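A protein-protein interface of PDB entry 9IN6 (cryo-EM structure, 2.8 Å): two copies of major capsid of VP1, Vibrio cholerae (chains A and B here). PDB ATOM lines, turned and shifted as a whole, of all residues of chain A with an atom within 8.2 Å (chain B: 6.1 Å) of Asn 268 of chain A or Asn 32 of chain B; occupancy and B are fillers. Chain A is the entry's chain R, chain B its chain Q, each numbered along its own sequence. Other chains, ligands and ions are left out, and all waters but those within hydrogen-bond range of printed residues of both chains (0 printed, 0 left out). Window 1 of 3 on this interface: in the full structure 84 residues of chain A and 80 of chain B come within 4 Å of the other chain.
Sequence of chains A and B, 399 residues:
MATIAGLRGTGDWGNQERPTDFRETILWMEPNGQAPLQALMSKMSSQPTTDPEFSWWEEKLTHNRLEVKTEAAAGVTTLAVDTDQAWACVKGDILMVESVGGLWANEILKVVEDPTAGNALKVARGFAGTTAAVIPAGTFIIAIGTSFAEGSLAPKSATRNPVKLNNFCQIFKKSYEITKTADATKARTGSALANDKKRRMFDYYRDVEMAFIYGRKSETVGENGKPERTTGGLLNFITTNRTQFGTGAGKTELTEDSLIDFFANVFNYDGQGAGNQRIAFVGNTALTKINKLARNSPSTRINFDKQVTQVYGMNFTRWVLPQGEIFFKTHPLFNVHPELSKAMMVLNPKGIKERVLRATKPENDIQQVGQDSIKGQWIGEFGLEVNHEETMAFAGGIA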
ATOM      1  N   LEU A  61       8.625 -13.955  11.943  1.00  0.00           N
ATOM      2  CA  LEU A  61       7.439 -13.649  12.733  1.00  0.00           C
ATOM      3  C   LEU A  61       7.739 -12.458  13.632  1.00  0.00           C
ATOM      4  O   LEU A  61       8.638 -12.525  14.475  1.00  0.00           O
ATOM      5  CB  LEU A  61       7.019 -14.856  13.568  1.00  0.00           C
ATOM      6  CG  LEU A  61       6.546 -16.091  12.802  1.00  0.00           C
ATOM      7  CD1 LEU A  61       6.520 -17.297  13.712  1.00  0.00           C
ATOM      8  CD2 LEU A  61       5.174 -15.850  12.204  1.00  0.00           C
ATOM      9  N   ASN A 241      24.354  -5.158   9.851  1.00  0.00           N
ATOM     10  CA  ASN A 241      25.334  -4.964  10.914  1.00  0.00           C
ATOM     11  C   ASN A 241      26.723  -4.871  10.291  1.00  0.00           C
ATOM     12  O   ASN A 241      27.452  -5.859  10.218  1.00  0.00           O
ATOM     13  CB  ASN A 241      25.264  -6.105  11.915  1.00  0.00           C
ATOM     14  CG  ASN A 241      23.997  -6.088  12.728  1.00  0.00           C
ATOM     15  OD1 ASN A 241      23.424  -5.031  12.982  1.00  0.00           O
ATOM     16  ND2 ASN A 241      23.551  -7.263  13.150  1.00  0.00           N
ATOM     17  N   PHE A 263      28.038  -5.114  19.278  1.00  0.00           N
ATOM     18  CA  PHE A 263      27.784  -6.535  19.479  1.00  0.00           C
ATOM     19  C   PHE A 263      26.345  -6.846  19.862  1.00  0.00           C
ATOM     20  O   PHE A 263      25.930  -8.002  19.752  1.00  0.00           O
ATOM     21  CB  PHE A 263      28.702  -7.081  20.569  1.00  0.00           C
ATOM     22  CG  PHE A 263      30.108  -7.303  20.125  1.00  0.00           C
ATOM     23  CD1 PHE A 263      30.405  -7.488  18.793  1.00  0.00           C
ATOM     24  CD2 PHE A 263      31.139  -7.329  21.044  1.00  0.00           C
ATOM     25  CE1 PHE A 263      31.699  -7.693  18.386  1.00  0.00           C
ATOM     26  CE2 PHE A 263      32.436  -7.536  20.643  1.00  0.00           C
ATOM     27  CZ  PHE A 263      32.718  -7.717  19.311  1.00  0.00           C
ATOM     28  N   ALA A 264      25.581  -5.854  20.317  1.00  0.00           N
ATOM     29  CA  ALA A 264      24.276  -6.147  20.899  1.00  0.00           C
ATOM     30  C   ALA A 264      23.233  -6.490  19.845  1.00  0.00           C
ATOM     31  O   ALA A 264      22.234  -7.148  20.158  1.00  0.00           O
ATOM     32  CB  ALA A 264      23.803  -4.965  21.741  1.00  0.00           C
ATOM     33  N   ASN A 265      23.440  -6.066  18.598  1.00  0.00           N
ATOM     34  CA  ASN A 265      22.396  -6.208  17.590  1.00  0.00           C
ATOM     35  C   ASN A 265      22.233  -7.647  17.119  1.00  0.00           C
ATOM     36  O   ASN A 265      21.155  -8.019  16.644  1.00  0.00           O
ATOM     37  CB  ASN A 265      22.697  -5.303  16.402  1.00  0.00           C
ATOM     38  CG  ASN A 265      22.931  -3.875  16.816  1.00  0.00           C
ATOM     39  OD1 ASN A 265      22.601  -3.482  17.932  1.00  0.00           O
ATOM     40  ND2 ASN A 265      23.513  -3.087  15.921  1.00  0.00           N
ATOM     41  N   VAL A 266      23.277  -8.472  17.240  1.00  0.00           N
ATOM     42  CA  VAL A 266      23.252  -9.804  16.638  1.00  0.00           C
ATOM     43  C   VAL A 266      22.460 -10.818  17.446  1.00  0.00           C
ATOM     44  O   VAL A 266      22.435 -11.997  17.077  1.00  0.00           O
ATOM     45  CB  VAL A 266      24.684 -10.333  16.432  1.00  0.00           C
ATOM     46  CG1 VAL A 266      25.512  -9.314  15.683  1.00  0.00           C
ATOM     47  CG2 VAL A 266      25.323 -10.657  17.756  1.00  0.00           C
ATOM     48  N   PHE A 267      21.806 -10.405  18.532  1.00  0.00           N
ATOM     49  CA  PHE A 267      21.130 -11.336  19.426  1.00  0.00           C
ATOM     50  C   PHE A 267      19.631 -11.084  19.527  1.00  0.00           C
ATOM     51  O   PHE A 267      18.981 -11.611  20.433  1.00  0.00           O
ATOM     52  CB  PHE A 267      21.762 -11.281  20.815  1.00  0.00           C
ATOM     53  CG  PHE A 267      23.108 -11.927  20.894  1.00  0.00           C
ATOM     54  CD1 PHE A 267      23.235 -13.298  20.810  1.00  0.00           C
ATOM     55  CD2 PHE A 267      24.246 -11.165  21.063  1.00  0.00           C
ATOM     56  CE1 PHE A 267      24.468 -13.895  20.883  1.00  0.00           C
ATOM     57  CE2 PHE A 267      25.483 -11.756  21.139  1.00  0.00           C
ATOM     58  CZ  PHE A 267      25.594 -13.122  21.048  1.00  0.00           C
ATOM     59  N   ASN A 268      19.063 -10.292  18.618  1.00  0.00           N
ATOM     60  CA  ASN A 268      17.647  -9.959  18.728  1.00  0.00           C
ATOM     61  C   ASN A 268      16.759 -11.131  18.332  1.00  0.00           C
ATOM     62  O   ASN A 268      15.723 -11.370  18.961  1.00  0.00           O
ATOM     63  CB  ASN A 268      17.327  -8.737  17.873  1.00  0.00           C
ATOM     64  CG  ASN A 268      17.689  -7.443  18.556  1.00  0.00           C
ATOM     65  OD1 ASN A 268      18.000  -7.422  19.745  1.00  0.00           O
ATOM     66  ND2 ASN A 268      17.648  -6.348  17.809  1.00  0.00           N
ATOM     67  N   TYR A 269      17.140 -11.867  17.295  1.00  0.00           N
ATOM     68  CA  TYR A 269      16.332 -12.952  16.760  1.00  0.00           C
ATOM     69  C   TYR A 269      17.022 -14.283  16.993  1.00  0.00           C
ATOM     70  O   TYR A 269      18.227 -14.417  16.768  1.00  0.00           O
ATOM     71  CB  TYR A 269      16.083 -12.764  15.265  1.00  0.00           C
ATOM     72  CG  TYR A 269      15.013 -11.757  14.936  1.00  0.00           C
ATOM     73  CD1 TYR A 269      13.681 -12.127  14.881  1.00  0.00           C
ATOM     74  CD2 TYR A 269      15.339 -10.441  14.664  1.00  0.00           C
ATOM     75  CE1 TYR A 269      12.702 -11.215  14.572  1.00  0.00           C
ATOM     76  CE2 TYR A 269      14.366  -9.520  14.357  1.00  0.00           C
ATOM     77  CZ  TYR A 269      13.048  -9.912  14.310  1.00  0.00           C
ATOM     78  OH  TYR A 269      12.070  -8.998  14.001  1.00  0.00           O
ATOM     79  N   ASP A 270      16.251 -15.274  17.438  1.00  0.00           N
ATOM     80  CA  ASP A 270      16.822 -16.591  17.688  1.00  0.00           C
ATOM     81  C   ASP A 270      17.211 -17.275  16.386  1.00  0.00           C
ATOM     82  O   ASP A 270      18.280 -17.884  16.295  1.00  0.00           O
ATOM     83  CB  ASP A 270      15.829 -17.450  18.470  1.00  0.00           C
ATOM     84  CG  ASP A 270      16.463 -18.697  19.062  1.00  0.00           C
ATOM     85  OD1 ASP A 270      15.919 -19.214  20.059  1.00  0.00           O
ATOM     86  OD2 ASP A 270      17.504 -19.162  18.553  1.00  0.00           O
ATOM     87  N   GLY A 271      16.368 -17.168  15.363  1.00  0.00           N
ATOM     88  CA  GLY A 271      16.633 -17.889  14.132  1.00  0.00           C
ATOM     89  C   GLY A 271      16.608 -19.387  14.367  1.00  0.00           C
ATOM     90  O   GLY A 271      15.675 -19.929  14.971  1.00  0.00           O
ATOM     91  N   ALA A 274      21.129 -20.738  16.435  1.00  0.00           N
ATOM     92  CA  ALA A 274      22.062 -19.651  16.710  1.00  0.00           C
ATOM     93  C   ALA A 274      22.483 -19.628  18.172  1.00  0.00           C
ATOM     94  O   ALA A 274      23.662 -19.414  18.480  1.00  0.00           O
ATOM     95  CB  ALA A 274      21.441 -18.316  16.307  1.00  0.00           C
ATOM     96  N   GLY A 275      21.544 -19.849  19.089  1.00  0.00           N
ATOM     97  CA  GLY A 275      21.895 -19.814  20.492  1.00  0.00           C
ATOM     98  C   GLY A 275      22.252 -18.412  20.954  1.00  0.00           C
ATOM     99  O   GLY A 275      21.709 -17.410  20.480  1.00  0.00           O
ATOM    100  N   ASN A 276      23.191 -18.343  21.899  1.00  0.00           N
ATOM    101  CA  ASN A 276      23.633 -17.070  22.456  1.00  0.00           C
ATOM    102  C   ASN A 276      25.150 -16.938  22.457  1.00  0.00           C
ATOM    103  O   ASN A 276      25.698 -16.184  23.265  1.00  0.00           O
ATOM    104  CB  ASN A 276      23.086 -16.882  23.871  1.00  0.00           C
ATOM    105  CG  ASN A 276      21.597 -16.619  23.887  1.00  0.00           C
ATOM    106  OD1 ASN A 276      21.133 -15.591  23.401  1.00  0.00           O
ATOM    107  ND2 ASN A 276      20.840 -17.550  24.449  1.00  0.00           N
ATOM    108  N   GLN A 277      25.842 -17.649  21.571  1.00  0.00           N
ATOM    109  CA  GLN A 277      27.287 -17.546  21.444  1.00  0.00           C
ATOM    110  C   GLN A 277      27.652 -17.318  19.988  1.00  0.00           C
ATOM    111  O   GLN A 277      26.928 -17.727  19.080  1.00  0.00           O
ATOM    112  CB  GLN A 277      27.988 -18.798  21.962  1.00  0.00           C
ATOM    113  CG  GLN A 277      27.903 -18.965  23.461  1.00  0.00           C
ATOM    114  CD  GLN A 277      27.857 -20.417  23.875  1.00  0.00           C
ATOM    115  OE1 GLN A 277      28.621 -21.241  23.376  1.00  0.00           O
ATOM    116  NE2 GLN A 277      26.950 -20.741  24.788  1.00  0.00           N
ATOM    117  N   ARG A 278      28.779 -16.643  19.773  1.00  0.00           N
ATOM    118  CA  ARG A 278      29.268 -16.362  18.433  1.00  0.00           C
ATOM    119  C   ARG A 278      30.778 -16.540  18.403  1.00  0.00           C
ATOM    120  O   ARG A 278      31.445 -16.546  19.438  1.00  0.00           O
ATOM    121  CB  ARG A 278      28.908 -14.946  17.975  1.00  0.00           C
ATOM    122  CG  ARG A 278      27.433 -14.624  18.011  1.00  0.00           C
ATOM    123  CD  ARG A 278      26.738 -15.073  16.748  1.00  0.00           C
ATOM    124  NE  ARG A 278      25.350 -14.632  16.719  1.00  0.00           N
ATOM    125  CZ  ARG A 278      24.354 -15.271  17.314  1.00  0.00           C
ATOM    126  NH1 ARG A 278      24.556 -16.393  17.982  1.00  0.00           N
ATOM    127  NH2 ARG A 278      23.125 -14.770  17.240  1.00  0.00           N
ATOM    128  N   GLN A 323      23.358  -9.947  26.634  1.00  0.00           N
ATOM    129  CA  GLN A 323      22.609 -10.709  25.645  1.00  0.00           C
ATOM    130  C   GLN A 323      23.295 -12.025  25.299  1.00  0.00           C
ATOM    131  O   GLN A 323      22.623 -13.046  25.126  1.00  0.00           O
ATOM    132  CB  GLN A 323      22.412  -9.875  24.381  1.00  0.00           C
ATOM    133  CG  GLN A 323      21.446  -8.724  24.544  1.00  0.00           C
ATOM    134  CD  GLN A 323      22.081  -7.524  25.205  1.00  0.00           C
ATOM    135  OE1 GLN A 323      23.242  -7.213  24.958  1.00  0.00           O
ATOM    136  NE2 GLN A 323      21.324  -6.843  26.053  1.00  0.00           N
ATOM    137  N   GLY A 324      24.613 -12.027  25.193  1.00  0.00           N
ATOM    138  CA  GLY A 324      25.317 -13.204  24.744  1.00  0.00           C
ATOM    139  C   GLY A 324      26.788 -13.170  25.071  1.00  0.00           C
ATOM    140  O   GLY A 324      27.211 -12.573  26.059  1.00  0.00           O
ATOM    141  N   GLU A 390      20.992 -11.218   9.936  1.00  0.00           N
ATOM    142  CA  GLU A 390      20.771 -10.385  11.112  1.00  0.00           C
ATOM    143  C   GLU A 390      21.527 -10.900  12.326  1.00  0.00           C
ATOM    144  O   GLU A 390      21.676 -10.164  13.305  1.00  0.00           O
ATOM    145  CB  GLU A 390      19.283 -10.306  11.438  1.00  0.00           C
ATOM    146  CG  GLU A 390      18.458  -9.576  10.401  1.00  0.00           C
ATOM    147  CD  GLU A 390      18.085 -10.471   9.236  1.00  0.00           C
ATOM    148  OE1 GLU A 390      18.422 -11.671   9.283  1.00  0.00           O
ATOM    149  OE2 GLU A 390      17.458  -9.977   8.276  1.00  0.00           O
ATOM    150  N   THR A 391      22.001 -12.140  12.284  1.00  0.00           N
ATOM    151  CA  THR A 391      22.751 -12.736  13.376  1.00  0.00           C
ATOM    152  C   THR A 391      24.256 -12.642  13.175  1.00  0.00           C
ATOM    153  O   THR A 391      25.007 -13.271  13.923  1.00  0.00           O
ATOM    154  CB  THR A 391      22.343 -14.198  13.552  1.00  0.00           C
ATOM    155  OG1 THR A 391      22.585 -14.909  12.334  1.00  0.00           O
ATOM    156  CG2 THR A 391      20.874 -14.294  13.888  1.00  0.00           C
ATOM    157  N   GLU B  30      12.473 -16.099  14.673  1.00  0.00           N
ATOM    158  CA  GLU B  30      11.579 -15.954  15.806  1.00  0.00           C
ATOM    159  C   GLU B  30      12.215 -15.056  16.859  1.00  0.00           C
ATOM    160  O   GLU B  30      13.440 -15.081  17.031  1.00  0.00           O
ATOM    161  CB  GLU B  30      11.260 -17.339  16.385  1.00  0.00           C
ATOM    162  CG  GLU B  30      10.271 -17.372  17.526  1.00  0.00           C
ATOM    163  CD  GLU B  30       9.985 -18.783  17.986  1.00  0.00           C
ATOM    164  OE1 GLU B  30      10.581 -19.721  17.418  1.00  0.00           O
ATOM    165  OE2 GLU B  30       9.163 -18.959  18.910  1.00  0.00           O
ATOM    166  N   PRO B  31      11.423 -14.242  17.558  1.00  0.00           N
ATOM    167  CA  PRO B  31      12.003 -13.338  18.558  1.00  0.00           C
ATOM    168  C   PRO B  31      12.720 -14.096  19.664  1.00  0.00           C
ATOM    169  O   PRO B  31      12.291 -15.170  20.090  1.00  0.00           O
ATOM    170  CB  PRO B  31      10.786 -12.578  19.094  1.00  0.00           C
ATOM    171  CG  PRO B  31       9.801 -12.647  18.002  1.00  0.00           C
ATOM    172  CD  PRO B  31       9.990 -13.981  17.360  1.00  0.00           C
ATOM    173  N   ASN B  32      13.816 -13.516  20.134  1.00  0.00           N
ATOM    174  CA  ASN B  32      14.654 -14.123  21.154  1.00  0.00           C
ATOM    175  C   ASN B  32      14.585 -13.311  22.439  1.00  0.00           C
ATOM    176  O   ASN B  32      14.588 -12.079  22.406  1.00  0.00           O
ATOM    177  CB  ASN B  32      16.103 -14.218  20.675  1.00  0.00           C
ATOM    178  CG  ASN B  32      16.963 -15.042  21.596  1.00  0.00           C
ATOM    179  OD1 ASN B  32      16.469 -15.911  22.310  1.00  0.00           O
ATOM    180  ND2 ASN B  32      18.260 -14.778  21.585  1.00  0.00           N
ATOM    181  N   GLY B  33      14.521 -14.007  23.566  1.00  0.00           N
ATOM    182  CA  GLY B  33      14.484 -13.343  24.855  1.00  0.00           C
ATOM    183  C   GLY B  33      14.564 -14.346  25.979  1.00  0.00           C
ATOM    184  O   GLY B  33      14.452 -15.557  25.768  1.00  0.00           O
ATOM    185  N   GLN B  34      14.769 -13.822  27.188  1.00  0.00           N
ATOM    186  CA  GLN B  34      14.872 -14.687  28.358  1.00  0.00           C
ATOM    187  C   GLN B  34      13.504 -15.182  28.810  1.00  0.00           C
ATOM    188  O   GLN B  34      13.370 -16.322  29.264  1.00  0.00           O
ATOM    189  CB  GLN B  34      15.578 -13.950  29.493  1.00  0.00           C
ATOM    190  CG  GLN B  34      17.008 -13.561  29.174  1.00  0.00           C
ATOM    191  CD  GLN B  34      17.565 -12.544  30.145  1.00  0.00           C
ATOM    192  OE1 GLN B  34      16.878 -12.106  31.062  1.00  0.00           O
ATOM    193  NE2 GLN B  34      18.820 -12.165  29.948  1.00  0.00           N
ATOM    194  N   ASN B 284      16.360  -5.224  25.455  1.00  0.00           N
ATOM    195  CA  ASN B 284      17.807  -5.409  25.473  1.00  0.00           C
ATOM    196  C   ASN B 284      18.535  -4.091  25.700  1.00  0.00           C
ATOM    197  O   ASN B 284      19.520  -4.039  26.448  1.00  0.00           O
ATOM    198  CB  ASN B 284      18.267  -6.060  24.174  1.00  0.00           C
ATOM    199  CG  ASN B 284      18.153  -7.565  24.210  1.00  0.00           C
ATOM    200  OD1 ASN B 284      18.122  -8.168  25.278  1.00  0.00           O
ATOM    201  ND2 ASN B 284      18.086  -8.181  23.040  1.00  0.00           N
ATOM    202  N   THR B 330      14.312 -10.104  30.203  1.00  0.00           N
ATOM    203  CA  THR B 330      14.069  -9.456  28.920  1.00  0.00           C
ATOM    204  C   THR B 330      12.856 -10.065  28.233  1.00  0.00           C
ATOM    205  O   THR B 330      12.745 -11.288  28.124  1.00  0.00           O
ATOM    206  CB  THR B 330      15.292  -9.568  28.013  1.00  0.00           C
ATOM    207  OG1 THR B 330      15.571 -10.948  27.760  1.00  0.00           O
ATOM    208  CG2 THR B 330      16.493  -8.925  28.667  1.00  0.00           C
ATOM    209  N   HIS B 331      11.958  -9.206  27.772  1.00  0.00           N
ATOM    210  CA  HIS B 331      10.734  -9.572  27.066  1.00  0.00           C
ATOM    211  C   HIS B 331      11.020  -9.752  25.582  1.00  0.00           C
ATOM    212  O   HIS B 331      11.560  -8.839  24.949  1.00  0.00           O
ATOM    213  CB  HIS B 331       9.672  -8.502  27.250  1.00  0.00           C
ATOM    214  CG  HIS B 331       8.282  -8.985  26.997  1.00  0.00           C
ATOM    215  ND1 HIS B 331       7.803  -9.241  25.731  1.00  0.00           N
ATOM    216  CD2 HIS B 331       7.260  -9.243  27.845  1.00  0.00           C
ATOM    217  CE1 HIS B 331       6.551  -9.647  25.811  1.00  0.00           C
ATOM    218  NE2 HIS B 331       6.194  -9.656  27.081  1.00  0.00           N
ATOM    219  N   PRO B 332      10.677 -10.902  24.996  1.00  0.00           N
ATOM    220  CA  PRO B 332      10.968 -11.105  23.566  1.00  0.00           C
ATOM    221  C   PRO B 332      10.322 -10.080  22.654  1.00  0.00           C
ATOM    222  O   PRO B 332      10.929  -9.684  21.654  1.00  0.00           O
ATOM    223  CB  PRO B 332      10.429 -12.517  23.304  1.00  0.00           C
ATOM    224  CG  PRO B 332      10.445 -13.174  24.630  1.00  0.00           C
ATOM    225  CD  PRO B 332      10.095 -12.102  25.611  1.00  0.00           C
ATOM    226  N   LEU B 333       9.103  -9.638  22.963  1.00  0.00           N
ATOM    227  CA  LEU B 333       8.444  -8.667  22.098  1.00  0.00           C
ATOM    228  C   LEU B 333       9.102  -7.297  22.183  1.00  0.00           C
ATOM    229  O   LEU B 333       9.132  -6.565  21.191  1.00  0.00           O
ATOM    230  CB  LEU B 333       6.962  -8.561  22.448  1.00  0.00           C
ATOM    231  CG  LEU B 333       6.084  -9.771  22.133  1.00  0.00           C
ATOM    232  CD1 LEU B 333       4.633  -9.440  22.407  1.00  0.00           C
ATOM    233  CD2 LEU B 333       6.269 -10.222  20.700  1.00  0.00           C
ATOM    234  N   ASN B 335      12.288  -6.776  22.589  1.00  0.00           N
ATOM    235  CA  ASN B 335      13.585  -6.819  21.922  1.00  0.00           C
ATOM    236  C   ASN B 335      13.465  -6.481  20.444  1.00  0.00           C
ATOM    237  O   ASN B 335      14.319  -5.782  19.888  1.00  0.00           O
ATOM    238  CB  ASN B 335      14.215  -8.198  22.101  1.00  0.00           C
ATOM    239  CG  ASN B 335      14.564  -8.491  23.538  1.00  0.00           C
ATOM    240  OD1 ASN B 335      14.698  -7.580  24.351  1.00  0.00           O
ATOM    241  ND2 ASN B 335      14.705  -9.767  23.863  1.00  0.00           N
ATOM    242  N   VAL B 336      12.418  -6.978  19.788  1.00  0.00           N
ATOM    243  CA  VAL B 336      12.297  -6.821  18.343  1.00  0.00           C
ATOM    244  C   VAL B 336      12.066  -5.362  17.970  1.00  0.00           C
ATOM    245  O   VAL B 336      12.727  -4.824  17.076  1.00  0.00           O
ATOM    246  CB  VAL B 336      11.172  -7.722  17.809  1.00  0.00           C
ATOM    247  CG1 VAL B 336      10.756  -7.276  16.428  1.00  0.00           C
ATOM    248  CG2 VAL B 336      11.626  -9.164  17.793  1.00  0.00           C
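O of Asn 32 of chain B lies within hydrogen-bond range of ND2 of Asn 335 of chain B, at 2.7 Å. The backbone NH of Asn 284 of chain B lies within hydrogen-bond range of the side-chain amide oxygen of Asn 335 of chain B (3.1 Å). The backbone carbonyl oxygen of His 331 of chain B sits close to the side-chain amide oxygen of Asn 335 of chain B (3.4 Å). OD1 of Asn 276 of chain A lies close to O of Gln 323 of chain A, 3.4 Å away.
Of the 20 printed residues of chain A, 8 touch a printed residue of chain B. Hydrophobic or aromatic side chains of chain A that line the printed part of chain B: Tyr 269. Along chain A the printed residues that touch a printed residue of chain B span positions 61 to 323. Printed residues of chain B that touch a printed residue of chain A: Glu 30, Pro 31, Asn 32, Asn 284, Asn 335 and Val 336. Along chain B the printed residues that touch a printed residue of chain A span positions 30 to 336. Among the printed residues, no Asp or Glu carboxylate lies within 4 Å of a Lys or Arg side-chain nitrogen of the other chain.
Asn 268 of chain A touches just these residues of chain B: Asn 32 (3.1 Å), Asn 284 (3.4 Å) and Asn 335 (3.97 Å). Of chain A, only Phe 267 (3.4 Å), Asn 268 (3.1 Å), Tyr 269 (3.8 Å), Asp 270 (3.4 Å) and Asn 276 (3.5 Å) come within 4 Å of Asn 32 of chain B. Of the printed residues of chain B, Leu 61 of chain A touches Pro 31 (3.5 Å). Of the printed residues of chain B, Asn 276 of chain A touches Asn 32. Printed residues of chain B within 4 Å of Gly 271 of chain A: Glu 30 (3.96 Å). Printed residues of chain A within 4 Å of Glu 30 of chain B: Tyr 269 (3.6 Å), Asp 270 (2.8 Å) and Gly 271 (3.96 Å). Of the printed residues of chain A, Val 336 of chain B touches Tyr 269 (3.3 Å). Asn 241 of chain A touches none of the printed residues of chain B. The nearest residue of chain A that does not touch Asn 32 of chain B is Gly 275 of chain A (4.5 Å). The nearest printed residue of chain B that does not touch Phe 267 of chain A is Asn 284 of chain B (4.4 Å).
Pro 31 of chain B touches Leu 61 of chain A (CD to O, 3.5 Å). Asn 268 of chain A touches Asn 335 of chain B (ND2 to O, 3.97 Å). Glu 30 of chain B touches Tyr 269 of chain A. Asn 32 of chain B touches Tyr 269 of chain A (CB to C, 3.8 Å). CG1 of Val 336 of chain B touches OH of Tyr 269 of chain A, 3.3 Å away. Asp 270 of chain A touches Asn 32 of chain B. Glu 30 of chain B touches Gly 271 of chain A (O to N, 3.96 Å).
No position is printed for both chains.
The backbone carbonyl oxygen of Glu 30 of chain B is in hydrogen-bond range of the backbone NH of Asp 270 of chain A, 2.8 Å away. ND2 of Asn 32 of chain B is in hydrogen-bond range of O of Phe 267 of chain A (3.4 Å). N of Asn 32 of chain B sits at hydrogen-bond distance from O of Asn 268 of chain A, at 3.1 Å. The side-chain amide nitrogen of Asn 32 of chain B lies within hydrogen-bond range of the side-chain amide oxygen of Asn 276 of chain A, 3.5 Å away. The side-chain amide nitrogen (ND2) of Asn 284 of chain B is in hydrogen-bond range of the side-chain amide oxygen (OD1) of Asn 268 of chain A (3.4 Å). O of Asn 284 of chain B is in hydrogen-bond range of NE2 of Gln 323 of chain A, at 3.4 Å.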
